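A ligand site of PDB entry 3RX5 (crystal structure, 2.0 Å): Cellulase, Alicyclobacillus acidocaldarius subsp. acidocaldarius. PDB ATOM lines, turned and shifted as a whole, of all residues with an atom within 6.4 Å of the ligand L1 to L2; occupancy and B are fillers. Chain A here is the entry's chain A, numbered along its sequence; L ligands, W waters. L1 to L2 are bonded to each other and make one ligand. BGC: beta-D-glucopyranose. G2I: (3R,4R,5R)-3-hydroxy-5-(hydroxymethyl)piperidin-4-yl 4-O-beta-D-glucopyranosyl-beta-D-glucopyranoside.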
ATOM      1  N   ALA A 144     -21.150  14.618 -23.085  1.00  0.00           N
ATOM      2  CA  ALA A 144     -20.180  13.554 -22.881  1.00  0.00           C
ATOM      3  C   ALA A 144     -19.178  13.868 -21.767  1.00  0.00           C
ATOM      4  O   ALA A 144     -19.579  14.078 -20.619  1.00  0.00           O
ATOM      5  CB  ALA A 144     -19.433  13.369 -24.228  1.00  0.00           C
ATOM      6  N   GLY A 145     -17.887  13.881 -22.108  1.00  0.00           N
ATOM      7  CA  GLY A 145     -16.816  14.253 -21.191  1.00  0.00           C
ATOM      8  C   GLY A 145     -16.665  15.772 -21.153  1.00  0.00           C
ATOM      9  O   GLY A 145     -16.008  16.302 -20.279  1.00  0.00           O
ATOM     10  N   ASP A 146     -17.302  16.479 -22.086  1.00  0.00           N
ATOM     11  CA  ASP A 146     -17.334  17.951 -22.150  1.00  0.00           C
ATOM     12  C   ASP A 146     -18.739  18.446 -21.735  1.00  0.00           C
ATOM     13  O   ASP A 146     -19.631  17.654 -21.497  1.00  0.00           O
ATOM     14  CB  ASP A 146     -16.969  18.428 -23.553  1.00  0.00           C
ATOM     15  CG  ASP A 146     -18.043  18.173 -24.583  1.00  0.00           C
ATOM     16  OD1 ASP A 146     -18.425  16.985 -24.751  1.00  0.00           O
ATOM     17  OD2 ASP A 146     -18.481  19.133 -25.234  1.00  0.00           O
ATOM     18  N   TYR A 150     -25.451  19.336 -27.757  1.00  0.00           N
ATOM     19  CA  TYR A 150     -25.513  19.244 -29.208  1.00  0.00           C
ATOM     20  C   TYR A 150     -26.789  18.539 -29.615  1.00  0.00           C
ATOM     21  O   TYR A 150     -27.053  17.429 -29.163  1.00  0.00           O
ATOM     22  CB  TYR A 150     -24.284  18.478 -29.746  1.00  0.00           C
ATOM     23  CG  TYR A 150     -22.945  18.887 -29.168  1.00  0.00           C
ATOM     24  CD1 TYR A 150     -22.519  18.407 -27.941  1.00  0.00           C
ATOM     25  CD2 TYR A 150     -22.059  19.653 -29.912  1.00  0.00           C
ATOM     26  CE1 TYR A 150     -21.250  18.717 -27.444  1.00  0.00           C
ATOM     27  CE2 TYR A 150     -20.802  19.999 -29.416  1.00  0.00           C
ATOM     28  CZ  TYR A 150     -20.388  19.504 -28.189  1.00  0.00           C
ATOM     29  OH  TYR A 150     -19.141  19.831 -27.733  1.00  0.00           O
ATOM     30  N   PHE A 221     -13.270  24.104 -25.586  1.00  0.00           N
ATOM     31  CA  PHE A 221     -13.281  23.128 -24.523  1.00  0.00           C
ATOM     32  C   PHE A 221     -12.497  23.660 -23.328  1.00  0.00           C
ATOM     33  O   PHE A 221     -11.371  24.120 -23.500  1.00  0.00           O
ATOM     34  CB  PHE A 221     -12.657  21.799 -24.957  1.00  0.00           C
ATOM     35  CG  PHE A 221     -13.444  21.050 -25.996  1.00  0.00           C
ATOM     36  CD1 PHE A 221     -14.724  20.589 -25.728  1.00  0.00           C
ATOM     37  CD2 PHE A 221     -12.880  20.771 -27.232  1.00  0.00           C
ATOM     38  CE1 PHE A 221     -15.437  19.858 -26.687  1.00  0.00           C
ATOM     39  CE2 PHE A 221     -13.577  20.015 -28.182  1.00  0.00           C
ATOM     40  CZ  PHE A 221     -14.848  19.571 -27.904  1.00  0.00           C
ATOM     41  N   PRO A 222     -13.058  23.562 -22.109  1.00  0.00           N
ATOM     42  CA  PRO A 222     -12.317  24.014 -20.928  1.00  0.00           C
ATOM     43  C   PRO A 222     -11.291  22.945 -20.527  1.00  0.00           C
ATOM     44  O   PRO A 222     -11.379  21.811 -21.031  1.00  0.00           O
ATOM     45  CB  PRO A 222     -13.399  24.173 -19.879  1.00  0.00           C
ATOM     46  CG  PRO A 222     -14.462  23.165 -20.275  1.00  0.00           C
ATOM     47  CD  PRO A 222     -14.394  23.031 -21.755  1.00  0.00           C
ATOM     48  N   PRO A 223     -10.351  23.218 -19.591  1.00  0.00           N
ATOM     49  CA  PRO A 223      -9.418  22.161 -19.175  1.00  0.00           C
ATOM     50  C   PRO A 223     -10.167  20.944 -18.661  1.00  0.00           C
ATOM     51  O   PRO A 223     -11.282  21.073 -18.155  1.00  0.00           O
ATOM     52  CB  PRO A 223      -8.603  22.836 -18.058  1.00  0.00           C
ATOM     53  CG  PRO A 223      -8.627  24.273 -18.410  1.00  0.00           C
ATOM     54  CD  PRO A 223     -10.042  24.484 -18.887  1.00  0.00           C
ATOM     55  N   LEU A 224      -9.556  19.757 -18.813  1.00  0.00           N
ATOM     56  CA  LEU A 224     -10.103  18.465 -18.364  1.00  0.00           C
ATOM     57  C   LEU A 224     -10.401  18.464 -16.862  1.00  0.00           C
ATOM     58  O   LEU A 224     -11.307  17.789 -16.389  1.00  0.00           O
ATOM     59  CB  LEU A 224      -9.129  17.315 -18.734  1.00  0.00           C
ATOM     60  CG  LEU A 224      -9.631  15.879 -18.547  1.00  0.00           C
ATOM     61  CD1 LEU A 224     -10.996  15.646 -19.237  1.00  0.00           C
ATOM     62  CD2 LEU A 224      -8.576  14.869 -19.023  1.00  0.00           C
ATOM     63  N   LEU A 296     -14.668  26.049 -31.285  1.00  0.00           N
ATOM     64  CA  LEU A 296     -13.774  24.902 -31.359  1.00  0.00           C
ATOM     65  C   LEU A 296     -14.331  23.619 -30.724  1.00  0.00           C
ATOM     66  O   LEU A 296     -13.613  22.632 -30.606  1.00  0.00           O
ATOM     67  CB  LEU A 296     -12.400  25.269 -30.751  1.00  0.00           C
ATOM     68  CG  LEU A 296     -11.723  26.519 -31.314  1.00  0.00           C
ATOM     69  CD1 LEU A 296     -10.483  26.881 -30.486  1.00  0.00           C
ATOM     70  CD2 LEU A 296     -11.355  26.334 -32.764  1.00  0.00           C
ATOM     71  N   GLY A 298     -17.228  20.322 -30.237  1.00  0.00           N
ATOM     72  CA  GLY A 298     -17.668  19.214 -31.087  1.00  0.00           C
ATOM     73  C   GLY A 298     -18.463  19.673 -32.292  1.00  0.00           C
ATOM     74  O   GLY A 298     -19.470  20.356 -32.142  1.00  0.00           O
ATOM     75  N   TRP A 401     -13.830   5.181 -33.436  1.00  0.00           N
ATOM     76  CA  TRP A 401     -14.235   6.040 -32.322  1.00  0.00           C
ATOM     77  C   TRP A 401     -15.688   5.669 -31.995  1.00  0.00           C
ATOM     78  O   TRP A 401     -16.517   5.628 -32.913  1.00  0.00           O
ATOM     79  CB  TRP A 401     -14.177   7.513 -32.756  1.00  0.00           C
ATOM     80  CG  TRP A 401     -14.156   8.489 -31.617  1.00  0.00           C
ATOM     81  CD1 TRP A 401     -14.993   8.538 -30.550  1.00  0.00           C
ATOM     82  CD2 TRP A 401     -13.310   9.645 -31.528  1.00  0.00           C
ATOM     83  NE1 TRP A 401     -14.690   9.615 -29.751  1.00  0.00           N
ATOM     84  CE2 TRP A 401     -13.677  10.332 -30.354  1.00  0.00           C
ATOM     85  CE3 TRP A 401     -12.337  10.210 -32.371  1.00  0.00           C
ATOM     86  CZ2 TRP A 401     -13.078  11.537 -29.971  1.00  0.00           C
ATOM     87  CZ3 TRP A 401     -11.707  11.379 -31.972  1.00  0.00           C
ATOM     88  CH2 TRP A 401     -12.100  12.048 -30.801  1.00  0.00           C
ATOM     89  N   HIS A 461     -12.378   9.845 -19.826  1.00  0.00           N
ATOM     90  CA  HIS A 461     -12.224  11.227 -20.243  1.00  0.00           C
ATOM     91  C   HIS A 461     -13.617  11.853 -19.951  1.00  0.00           C
ATOM     92  O   HIS A 461     -14.472  11.886 -20.829  1.00  0.00           O
ATOM     93  CB  HIS A 461     -11.848  11.319 -21.724  1.00  0.00           C
ATOM     94  CG  HIS A 461     -11.531  12.709 -22.184  1.00  0.00           C
ATOM     95  ND1 HIS A 461     -10.232  13.210 -22.127  1.00  0.00           N
ATOM     96  CD2 HIS A 461     -12.349  13.671 -22.663  1.00  0.00           C
ATOM     97  CE1 HIS A 461     -10.308  14.444 -22.604  1.00  0.00           C
ATOM     98  NE2 HIS A 461     -11.564  14.771 -22.928  1.00  0.00           N
ATOM     99  N   ARG A 463     -14.987  15.207 -17.568  1.00  0.00           N
ATOM    100  CA  ARG A 463     -14.634  16.335 -16.703  1.00  0.00           C
ATOM    101  C   ARG A 463     -15.110  16.234 -15.258  1.00  0.00           C
ATOM    102  O   ARG A 463     -14.227  16.294 -14.394  1.00  0.00           O
ATOM    103  CB  ARG A 463     -14.913  17.708 -17.354  1.00  0.00           C
ATOM    104  CG  ARG A 463     -13.910  18.065 -18.449  1.00  0.00           C
ATOM    105  CD  ARG A 463     -14.298  19.306 -19.247  1.00  0.00           C
ATOM    106  NE  ARG A 463     -13.304  19.620 -20.281  1.00  0.00           N
ATOM    107  CZ  ARG A 463     -13.160  18.961 -21.427  1.00  0.00           C
ATOM    108  NH1 ARG A 463     -13.925  17.917 -21.701  1.00  0.00           N
ATOM    109  NH2 ARG A 463     -12.220  19.321 -22.295  1.00  0.00           N
ATOM    110  N   GLN A 487      -6.685   8.141 -32.505  1.00  0.00           N
ATOM    111  CA  GLN A 487      -7.109   9.521 -32.654  1.00  0.00           C
ATOM    112  C   GLN A 487      -6.896  10.482 -31.481  1.00  0.00           C
ATOM    113  O   GLN A 487      -7.581  11.496 -31.384  1.00  0.00           O
ATOM    114  CB  GLN A 487      -8.496   9.616 -33.310  1.00  0.00           C
ATOM    115  CG  GLN A 487      -8.529   9.036 -34.735  1.00  0.00           C
ATOM    116  CD  GLN A 487      -9.911   8.831 -35.277  1.00  0.00           C
ATOM    117  OE1 GLN A 487     -10.747   8.151 -34.667  1.00  0.00           O
ATOM    118  NE2 GLN A 487     -10.152   9.288 -36.500  1.00  0.00           N
ATOM    119  N   GLN A 508      -7.289   8.985 -18.747  1.00  0.00           N
ATOM    120  CA  GLN A 508      -8.161  10.176 -18.795  1.00  0.00           C
ATOM    121  C   GLN A 508      -7.955  11.043 -20.024  1.00  0.00           C
ATOM    122  O   GLN A 508      -8.852  11.787 -20.389  1.00  0.00           O
ATOM    123  CB  GLN A 508      -8.031  10.999 -17.506  1.00  0.00           C
ATOM    124  CG  GLN A 508      -6.659  11.648 -17.346  1.00  0.00           C
ATOM    125  CD  GLN A 508      -6.562  12.562 -16.152  1.00  0.00           C
ATOM    126  OE1 GLN A 508      -6.903  12.205 -15.036  1.00  0.00           O
ATOM    127  NE2 GLN A 508      -6.012  13.751 -16.374  1.00  0.00           N
ATOM    128  N   ASP A 509      -6.759  10.989 -20.631  1.00  0.00           N
ATOM    129  CA  ASP A 509      -6.454  11.826 -21.773  1.00  0.00           C
ATOM    130  C   ASP A 509      -6.791  11.134 -23.063  1.00  0.00           C
ATOM    131  O   ASP A 509      -6.744  11.758 -24.109  1.00  0.00           O
ATOM    132  CB  ASP A 509      -4.984  12.290 -21.735  1.00  0.00           C
ATOM    133  CG  ASP A 509      -4.690  13.250 -20.592  1.00  0.00           C
ATOM    134  OD1 ASP A 509      -5.489  14.203 -20.384  1.00  0.00           O
ATOM    135  OD2 ASP A 509      -3.638  13.080 -19.936  1.00  0.00           O
ATOM    136  N   TYR A 511      -9.291  10.563 -25.121  1.00  0.00           N
ATOM    137  CA  TYR A 511     -10.680  10.870 -25.486  1.00  0.00           C
ATOM    138  C   TYR A 511     -11.189  10.061 -26.669  1.00  0.00           C
ATOM    139  O   TYR A 511     -12.403   9.916 -26.818  1.00  0.00           O
ATOM    140  CB  TYR A 511     -10.855  12.381 -25.737  1.00  0.00           C
ATOM    141  CG  TYR A 511      -9.835  12.985 -26.672  1.00  0.00           C
ATOM    142  CD1 TYR A 511      -9.981  12.897 -28.051  1.00  0.00           C
ATOM    143  CD2 TYR A 511      -8.732  13.676 -26.181  1.00  0.00           C
ATOM    144  CE1 TYR A 511      -9.055  13.488 -28.924  1.00  0.00           C
ATOM    145  CE2 TYR A 511      -7.822  14.293 -27.033  1.00  0.00           C
ATOM    146  CZ  TYR A 511      -7.983  14.192 -28.403  1.00  0.00           C
ATOM    147  OH  TYR A 511      -7.075  14.772 -29.257  1.00  0.00           O
ATOM    148  N   GLU A 515     -13.686   8.217 -23.777  1.00  0.00           N
ATOM    149  CA  GLU A 515     -14.691   9.224 -23.414  1.00  0.00           C
ATOM    150  C   GLU A 515     -15.994   8.470 -23.169  1.00  0.00           C
ATOM    151  O   GLU A 515     -16.092   7.281 -23.451  1.00  0.00           O
ATOM    152  CB  GLU A 515     -14.883  10.288 -24.532  1.00  0.00           C
ATOM    153  CG  GLU A 515     -15.546  11.559 -24.000  1.00  0.00           C
ATOM    154  CD  GLU A 515     -15.359  12.860 -24.751  1.00  0.00           C
ATOM    155  OE1 GLU A 515     -14.819  12.846 -25.885  1.00  0.00           O
ATOM    156  OE2 GLU A 515     -15.773  13.902 -24.214  1.00  0.00           O
HETATM  157  C2  BGC L   1      -7.425  19.448 -27.019  1.00  0.00           C
HETATM  158  C3  BGC L   1      -8.936  19.199 -26.917  1.00  0.00           C
HETATM  159  C4  BGC L   1      -9.252  18.228 -25.779  1.00  0.00           C
HETATM  160  C5  BGC L   1      -8.587  18.742 -24.506  1.00  0.00           C
HETATM  161  C6  BGC L   1      -8.846  17.880 -23.271  1.00  0.00           C
HETATM  162  C1  BGC L   1      -6.906  19.901 -25.655  1.00  0.00           C
HETATM  163  O1  BGC L   1      -5.490  20.164 -25.617  1.00  0.00           O
HETATM  164  O2  BGC L   1      -7.191  20.449 -28.017  1.00  0.00           O
HETATM  165  O3  BGC L   1      -9.475  18.750 -28.170  1.00  0.00           O
HETATM  166  O4  BGC L   1     -10.651  18.226 -25.543  1.00  0.00           O
HETATM  167  O5  BGC L   1      -7.185  18.859 -24.724  1.00  0.00           O
HETATM  168  O6  BGC L   1      -8.216  16.614 -23.484  1.00  0.00           O
HETATM  169  C2  BGC L   2     -12.697  17.072 -25.313  1.00  0.00           C
HETATM  170  C3  BGC L   2     -13.527  15.886 -25.784  1.00  0.00           C
HETATM  171  C4  BGC L   2     -13.601  15.933 -27.291  1.00  0.00           C
HETATM  172  C5  BGC L   2     -12.251  16.049 -27.991  1.00  0.00           C
HETATM  173  C6  BGC L   2     -12.578  16.549 -29.397  1.00  0.00           C
HETATM  174  C1  BGC L   2     -11.311  17.030 -25.955  1.00  0.00           C
HETATM  175  O2  BGC L   2     -12.575  17.037 -23.890  1.00  0.00           O
HETATM  176  O3  BGC L   2     -14.870  16.021 -25.310  1.00  0.00           O
HETATM  177  O4  BGC L   2     -14.249  14.740 -27.753  1.00  0.00           O
HETATM  178  O5  BGC L   2     -11.437  17.055 -27.387  1.00  0.00           O
HETATM  179  O6  BGC L   2     -11.604  16.053 -30.301  1.00  0.00           O
HETATM  180  O61 G2I L   3     -16.058  11.681 -28.130  1.00  0.00           O
HETATM  181  C61 G2I L   3     -17.464  11.788 -27.806  1.00  0.00           C
HETATM  182  C51 G2I L   3     -17.937  13.233 -28.090  1.00  0.00           C
HETATM  183  C71 G2I L   3     -17.485  14.192 -26.905  1.00  0.00           C
HETATM  184  N11 G2I L   3     -18.239  15.494 -27.010  1.00  0.00           N
HETATM  185  C21 G2I L   3     -17.538  16.214 -28.176  1.00  0.00           C
HETATM  186  C31 G2I L   3     -17.990  15.382 -29.465  1.00  0.00           C
HETATM  187  O31 G2I L   3     -17.452  15.913 -30.642  1.00  0.00           O
HETATM  188  C41 G2I L   3     -17.459  13.888 -29.451  1.00  0.00           C
HETATM  189  O41 G2I L   3     -18.151  13.204 -30.553  1.00  0.00           O
HETATM  190  C12 G2I L   3     -17.304  12.336 -31.246  1.00  0.00           C
HETATM  191  C22 G2I L   3     -18.149  11.352 -32.130  1.00  0.00           C
HETATM  192  O22 G2I L   3     -18.680  10.517 -31.177  1.00  0.00           O
HETATM  193  C32 G2I L   3     -17.132  10.615 -33.051  1.00  0.00           C
HETATM  194  O32 G2I L   3     -17.888   9.738 -33.967  1.00  0.00           O
HETATM  195  O52 G2I L   3     -16.537  13.213 -32.102  1.00  0.00           O
HETATM  196  C52 G2I L   3     -15.529  12.561 -32.854  1.00  0.00           C
HETATM  197  C62 G2I L   3     -14.357  13.640 -33.221  1.00  0.00           C
HETATM  198  O62 G2I L   3     -14.953  14.390 -34.227  1.00  0.00           O
HETATM  199  C42 G2I L   3     -16.236  11.695 -33.887  1.00  0.00           C
HETATM  200  O42 G2I L   3     -15.164  10.944 -34.238  1.00  0.00           O
HETATM  201  C13 G2I L   3     -15.207  10.437 -35.544  1.00  0.00           C
HETATM  202  C23 G2I L   3     -13.764  10.141 -36.250  1.00  0.00           C
HETATM  203  O23 G2I L   3     -13.089  11.203 -36.345  1.00  0.00           O
HETATM  204  C33 G2I L   3     -13.776   9.466 -37.594  1.00  0.00           C
HETATM  205  O33 G2I L   3     -12.490   8.965 -37.998  1.00  0.00           O
HETATM  206  C43 G2I L   3     -14.700   8.246 -37.477  1.00  0.00           C
HETATM  207  O43 G2I L   3     -14.957   7.940 -38.794  1.00  0.00           O
HETATM  208  O53 G2I L   3     -15.890   9.187 -35.556  1.00  0.00           O
HETATM  209  C53 G2I L   3     -16.147   8.661 -36.875  1.00  0.00           C
HETATM  210  C63 G2I L   3     -17.230   7.519 -36.809  1.00  0.00           C
HETATM  211  O63 G2I L   3     -18.223   7.863 -35.864  1.00  0.00           O
HETATM  212  O   HOH W   1     -14.889  16.521 -31.529  1.00  0.00           O
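ND1 of His 461 is in hydrogen-bond range of O of Gln 508, 2.6 Å away. The side-chain hydroxyl (OH) of Tyr 150 sits at hydrogen-bond distance from the side-chain carboxylate (OD2) of Asp 146, at 2.7 Å. The guanidinium group (NH1) of Arg 463 sits at hydrogen-bond distance from the backbone carbonyl oxygen (O) of Gly 145 (3.0 Å). The side-chain carboxylate (OE2) of Glu 515 is in hydrogen-bond range of the backbone NH (N) of Gly 145 (3.0 Å). The guanidinium group (NE) of Arg 463 lies within hydrogen-bond range of the backbone carbonyl oxygen (O) of Pro 223 (3.3 Å). NH2 of Arg 463 is in hydrogen-bond range of O of Pro 222, at 2.9 Å.
Merely in contact with the ligand L1 to L2: Asp 146 (3.6 Å), Phe 221 (3.7 Å) and Tyr 511 (3.9 Å). Hydrophobic or aromatic side chains that line the ligand L1 to L2: Phe 221, His 461 and Tyr 511. Six residues have an atom within 4 Å of the ligand L1 to L2: Asp 146, Phe 221, His 461, Arg 463, Tyr 511 and Glu 515.
O61 of G2I L3 is in hydrogen-bond range of OE1 of Glu 515 (2.8 Å). NE2 of His 461 is in hydrogen-bond range of O2 of BGC L2 (2.7 Å). NE2 of Gln 487 sits at hydrogen-bond distance from O33 of G2I L3, 2.8 Å away. O2 of BGC L2 is in hydrogen-bond range of NH1 of Arg 463 (2.7 Å). A nitrogen (N11) of G2I L3 lies within salt-bridge range of the side-chain carboxylate (OD1) of Asp 146 (2.7 Å). NE1 of Trp 401 is in hydrogen-bond range of O61 of G2I L3 (3.0 Å). The side-chain carboxylate of Glu 515 sits at hydrogen-bond distance from an oxygen (O3) of BGC L2, at 2.6 Å.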
